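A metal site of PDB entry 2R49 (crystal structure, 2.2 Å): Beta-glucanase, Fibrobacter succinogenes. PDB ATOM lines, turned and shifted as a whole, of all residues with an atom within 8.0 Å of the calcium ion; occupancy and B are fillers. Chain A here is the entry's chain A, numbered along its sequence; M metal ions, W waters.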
ATOM      1  N   ARG A  24      12.264 -11.088  12.405  1.00  0.00           N
ATOM      2  CA  ARG A  24      12.597 -10.649  11.062  1.00  0.00           C
ATOM      3  C   ARG A  24      14.092 -10.782  10.952  1.00  0.00           C
ATOM      4  O   ARG A  24      14.835 -10.041  11.592  1.00  0.00           O
ATOM      5  CB  ARG A  24      12.166  -9.191  10.916  1.00  0.00           C
ATOM      6  CG  ARG A  24      12.532  -8.549   9.599  1.00  0.00           C
ATOM      7  CD  ARG A  24      11.774  -9.230   8.490  1.00  0.00           C
ATOM      8  NE  ARG A  24      11.913  -8.547   7.217  1.00  0.00           N
ATOM      9  CZ  ARG A  24      11.285  -8.954   6.113  1.00  0.00           C
ATOM     10  NH1 ARG A  24      10.498 -10.025   6.151  1.00  0.00           N
ATOM     11  NH2 ARG A  24      11.463  -8.283   4.978  1.00  0.00           N
ATOM     12  N   ILE A 161      19.175  -9.780  13.104  1.00  0.00           N
ATOM     13  CA  ILE A 161      17.799  -9.805  13.542  1.00  0.00           C
ATOM     14  C   ILE A 161      17.342  -8.328  13.596  1.00  0.00           C
ATOM     15  O   ILE A 161      17.878  -7.528  14.358  1.00  0.00           O
ATOM     16  CB  ILE A 161      17.649 -10.507  14.944  1.00  0.00           C
ATOM     17  CG1 ILE A 161      18.304 -11.908  14.925  1.00  0.00           C
ATOM     18  CG2 ILE A 161      16.202 -10.689  15.248  1.00  0.00           C
ATOM     19  CD1 ILE A 161      17.986 -12.739  16.198  1.00  0.00           C
ATOM     20  N   ASN A 162      16.384  -7.983  12.748  1.00  0.00           N
ATOM     21  CA  ASN A 162      15.879  -6.612  12.687  1.00  0.00           C
ATOM     22  C   ASN A 162      14.905  -6.387  13.857  1.00  0.00           C
ATOM     23  O   ASN A 162      15.079  -5.455  14.602  1.00  0.00           O
ATOM     24  CB  ASN A 162      15.204  -6.360  11.339  1.00  0.00           C
ATOM     25  CG  ASN A 162      15.069  -4.864  10.999  1.00  0.00           C
ATOM     26  OD1 ASN A 162      15.494  -3.979  11.760  1.00  0.00           O
ATOM     27  ND2 ASN A 162      14.489  -4.582   9.846  1.00  0.00           N
ATOM     28  N   TRP A 163      13.935  -7.266  14.032  1.00  0.00           N
ATOM     29  CA  TRP A 163      12.995  -7.148  15.135  1.00  0.00           C
ATOM     30  C   TRP A 163      12.317  -8.472  15.507  1.00  0.00           C
ATOM     31  O   TRP A 163      12.281  -9.430  14.739  1.00  0.00           O
ATOM     32  CB  TRP A 163      11.874  -6.116  14.847  1.00  0.00           C
ATOM     33  CG  TRP A 163      11.172  -6.264  13.520  1.00  0.00           C
ATOM     34  CD1 TRP A 163      11.430  -5.543  12.369  1.00  0.00           C
ATOM     35  CD2 TRP A 163      10.113  -7.191  13.178  1.00  0.00           C
ATOM     36  NE1 TRP A 163      10.594  -5.983  11.344  1.00  0.00           N
ATOM     37  CE2 TRP A 163       9.786  -6.980  11.817  1.00  0.00           C
ATOM     38  CE3 TRP A 163       9.404  -8.163  13.894  1.00  0.00           C
ATOM     39  CZ2 TRP A 163       8.801  -7.709  11.164  1.00  0.00           C
ATOM     40  CZ3 TRP A 163       8.415  -8.900  13.230  1.00  0.00           C
ATOM     41  CH2 TRP A 163       8.125  -8.666  11.901  1.00  0.00           C
ATOM     42  N   VAL A 164      11.719  -8.462  16.693  1.00  0.00           N
ATOM     43  CA  VAL A 164      10.983  -9.600  17.226  1.00  0.00           C
ATOM     44  C   VAL A 164       9.684  -9.039  17.784  1.00  0.00           C
ATOM     45  O   VAL A 164       9.671  -7.960  18.359  1.00  0.00           O
ATOM     46  CB  VAL A 164      11.812 -10.300  18.354  1.00  0.00           C
ATOM     47  CG1 VAL A 164      10.946 -11.259  19.213  1.00  0.00           C
ATOM     48  CG2 VAL A 164      12.974 -11.054  17.716  1.00  0.00           C
ATOM     49  N   ASP A 186      10.419  -5.757  19.856  1.00  0.00           N
ATOM     50  CA  ASP A 186      11.770  -5.283  20.142  1.00  0.00           C
ATOM     51  C   ASP A 186      12.392  -4.948  18.784  1.00  0.00           C
ATOM     52  O   ASP A 186      12.566  -5.823  17.956  1.00  0.00           O
ATOM     53  CB  ASP A 186      12.609  -6.349  20.872  1.00  0.00           C
ATOM     54  CG  ASP A 186      13.871  -5.764  21.542  1.00  0.00           C
ATOM     55  OD1 ASP A 186      14.374  -4.734  21.032  1.00  0.00           O
ATOM     56  OD2 ASP A 186      14.362  -6.327  22.556  1.00  0.00           O
ATOM     57  N   ASN A 187      12.702  -3.675  18.572  1.00  0.00           N
ATOM     58  CA  ASN A 187      13.333  -3.218  17.335  1.00  0.00           C
ATOM     59  C   ASN A 187      14.865  -3.220  17.410  1.00  0.00           C
ATOM     60  O   ASN A 187      15.533  -2.808  16.456  1.00  0.00           O
ATOM     61  CB  ASN A 187      12.821  -1.834  16.963  1.00  0.00           C
ATOM     62  CG  ASN A 187      11.429  -1.886  16.358  1.00  0.00           C
ATOM     63  OD1 ASN A 187      11.180  -2.654  15.429  1.00  0.00           O
ATOM     64  ND2 ASN A 187      10.514  -1.066  16.877  1.00  0.00           N
ATOM     65  N   PHE A 188      15.399  -3.651  18.560  1.00  0.00           N
ATOM     66  CA  PHE A 188      16.839  -3.770  18.731  1.00  0.00           C
ATOM     67  C   PHE A 188      17.753  -2.556  18.546  1.00  0.00           C
ATOM     68  O   PHE A 188      18.853  -2.644  17.987  1.00  0.00           O
ATOM     69  CB  PHE A 188      17.341  -4.946  17.872  1.00  0.00           C
ATOM     70  CG  PHE A 188      16.791  -6.283  18.327  1.00  0.00           C
ATOM     71  CD1 PHE A 188      16.029  -7.085  17.462  1.00  0.00           C
ATOM     72  CD2 PHE A 188      16.941  -6.690  19.656  1.00  0.00           C
ATOM     73  CE1 PHE A 188      15.426  -8.255  17.931  1.00  0.00           C
ATOM     74  CE2 PHE A 188      16.329  -7.870  20.127  1.00  0.00           C
ATOM     75  CZ  PHE A 188      15.576  -8.641  19.273  1.00  0.00           C
ATOM     76  N   ASP A 189      17.295  -1.401  19.012  1.00  0.00           N
ATOM     77  CA  ASP A 189      18.136  -0.227  18.961  1.00  0.00           C
ATOM     78  C   ASP A 189      19.194  -0.406  20.061  1.00  0.00           C
ATOM     79  O   ASP A 189      20.222   0.264  20.092  1.00  0.00           O
ATOM     80  CB  ASP A 189      17.298   1.000  19.240  1.00  0.00           C
ATOM     81  CG  ASP A 189      17.700   2.151  18.385  1.00  0.00           C
ATOM     82  OD1 ASP A 189      16.996   2.355  17.350  1.00  0.00           O
ATOM     83  OD2 ASP A 189      18.722   2.818  18.724  1.00  0.00           O
ATOM     84  N   ARG A 218      23.699  -3.303  16.642  1.00  0.00           N
ATOM     85  CA  ARG A 218      24.478  -2.458  15.745  1.00  0.00           C
ATOM     86  C   ARG A 218      23.549  -1.832  14.704  1.00  0.00           C
ATOM     87  O   ARG A 218      22.911  -2.555  13.950  1.00  0.00           O
ATOM     88  CB  ARG A 218      25.535  -3.283  14.974  1.00  0.00           C
ATOM     89  CG  ARG A 218      26.892  -3.393  15.645  1.00  0.00           C
ATOM     90  CD  ARG A 218      27.690  -2.098  15.472  1.00  0.00           C
ATOM     91  NE  ARG A 218      28.476  -2.219  14.282  1.00  0.00           N
ATOM     92  CZ  ARG A 218      29.580  -2.947  14.186  1.00  0.00           C
ATOM     93  NH1 ARG A 218      30.066  -3.642  15.222  1.00  0.00           N
ATOM     94  NH2 ARG A 218      30.173  -3.034  13.011  1.00  0.00           N
ATOM     95  N   ASP A 219      23.509  -0.512  14.650  1.00  0.00           N
ATOM     96  CA  ASP A 219      22.693   0.189  13.663  1.00  0.00           C
ATOM     97  C   ASP A 219      21.233  -0.207  13.664  1.00  0.00           C
ATOM     98  O   ASP A 219      20.612  -0.285  12.591  1.00  0.00           O
ATOM     99  CB  ASP A 219      23.249  -0.068  12.247  1.00  0.00           C
ATOM    100  CG  ASP A 219      24.543   0.684  11.956  1.00  0.00           C
ATOM    101  OD1 ASP A 219      25.008   0.596  10.801  1.00  0.00           O
ATOM    102  OD2 ASP A 219      25.095   1.360  12.854  1.00  0.00           O
ATOM    103  N   GLY A 220      20.659  -0.486  14.823  1.00  0.00           N
ATOM    104  CA  GLY A 220      19.248  -0.854  14.792  1.00  0.00           C
ATOM    105  C   GLY A 220      18.929  -2.304  14.460  1.00  0.00           C
ATOM    106  O   GLY A 220      17.772  -2.655  14.241  1.00  0.00           O
ATOM    107  N   MET A 221      19.949  -3.143  14.433  1.00  0.00           N
ATOM    108  CA  MET A 221      19.780  -4.555  14.203  1.00  0.00           C
ATOM    109  C   MET A 221      20.562  -5.314  15.265  1.00  0.00           C
ATOM    110  O   MET A 221      21.608  -4.864  15.730  1.00  0.00           O
ATOM    111  CB  MET A 221      20.309  -4.944  12.810  1.00  0.00           C
ATOM    112  CG  MET A 221      19.476  -4.343  11.680  1.00  0.00           C
ATOM    113  SD  MET A 221      18.968  -5.569  10.489  1.00  0.00           S
ATOM    114  CE  MET A 221      18.448  -4.479   9.076  1.00  0.00           C
ATOM    115  N   LEU A 222      20.042  -6.477  15.656  1.00  0.00           N
ATOM    116  CA  LEU A 222      20.759  -7.276  16.627  1.00  0.00           C
ATOM    117  C   LEU A 222      21.647  -8.151  15.754  1.00  0.00           C
ATOM    118  O   LEU A 222      21.222  -8.632  14.697  1.00  0.00           O
ATOM    119  CB  LEU A 222      19.790  -8.150  17.434  1.00  0.00           C
ATOM    120  CG  LEU A 222      20.232  -8.577  18.852  1.00  0.00           C
ATOM    121  CD1 LEU A 222      19.661  -9.984  19.208  1.00  0.00           C
ATOM    122  CD2 LEU A 222      21.723  -8.651  18.913  1.00  0.00           C
ATOM    123  N   ASP A 241      17.131  -3.812   5.220  1.00  0.00           N
ATOM    124  CA  ASP A 241      15.948  -4.638   5.128  1.00  0.00           C
ATOM    125  C   ASP A 241      14.930  -3.761   4.427  1.00  0.00           C
ATOM    126  O   ASP A 241      14.438  -2.836   5.035  1.00  0.00           O
ATOM    127  CB  ASP A 241      15.411  -5.037   6.513  1.00  0.00           C
ATOM    128  CG  ASP A 241      14.152  -5.910   6.424  1.00  0.00           C
ATOM    129  OD1 ASP A 241      13.580  -6.267   7.490  1.00  0.00           O
ATOM    130  OD2 ASP A 241      13.739  -6.242   5.284  1.00  0.00           O
HETATM  131 CA    CA M   1      15.416  -3.072  13.968  1.00  0.00          CA
HETATM  132  O   HOH W   1      16.002  -0.080  15.684  1.00  0.00           O
HETATM  133  O   HOH W   2      13.219  -2.655  13.502  1.00  0.00           O
HETATM  134  O   HOH W   3      15.471  -0.610  13.171  1.00  0.00           O
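The backbone NH of Asn 162 is in hydrogen-bond range of the backbone carbonyl oxygen of Arg 24 (2.8 Å).
The side-chain amide nitrogen (ND2) of Asn 162 is in hydrogen-bond range of the side-chain carboxylate (OD1) of Asp 241.
Three residues have an atom within 4 Å of the calcium ion: Asn 162, Asn 187 and Gly 220.
Along chain A the residues within 4 Å of the calcium ion span positions 162 to 220.
The nearest printed residue that does not touch the calcium ion is Trp 163 (4.4 Å).
The calcium ion is bound by water W2 (2.3 Å), OD1 of Asn 162 (2.4 Å), O of Gly 220 (2.4 Å), O of Asn 162 (2.5 Å), O of Asn 187 (2.5 Å) and water W3 (2.6 Å).
The calcium ion has six donor atoms within binding distance.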
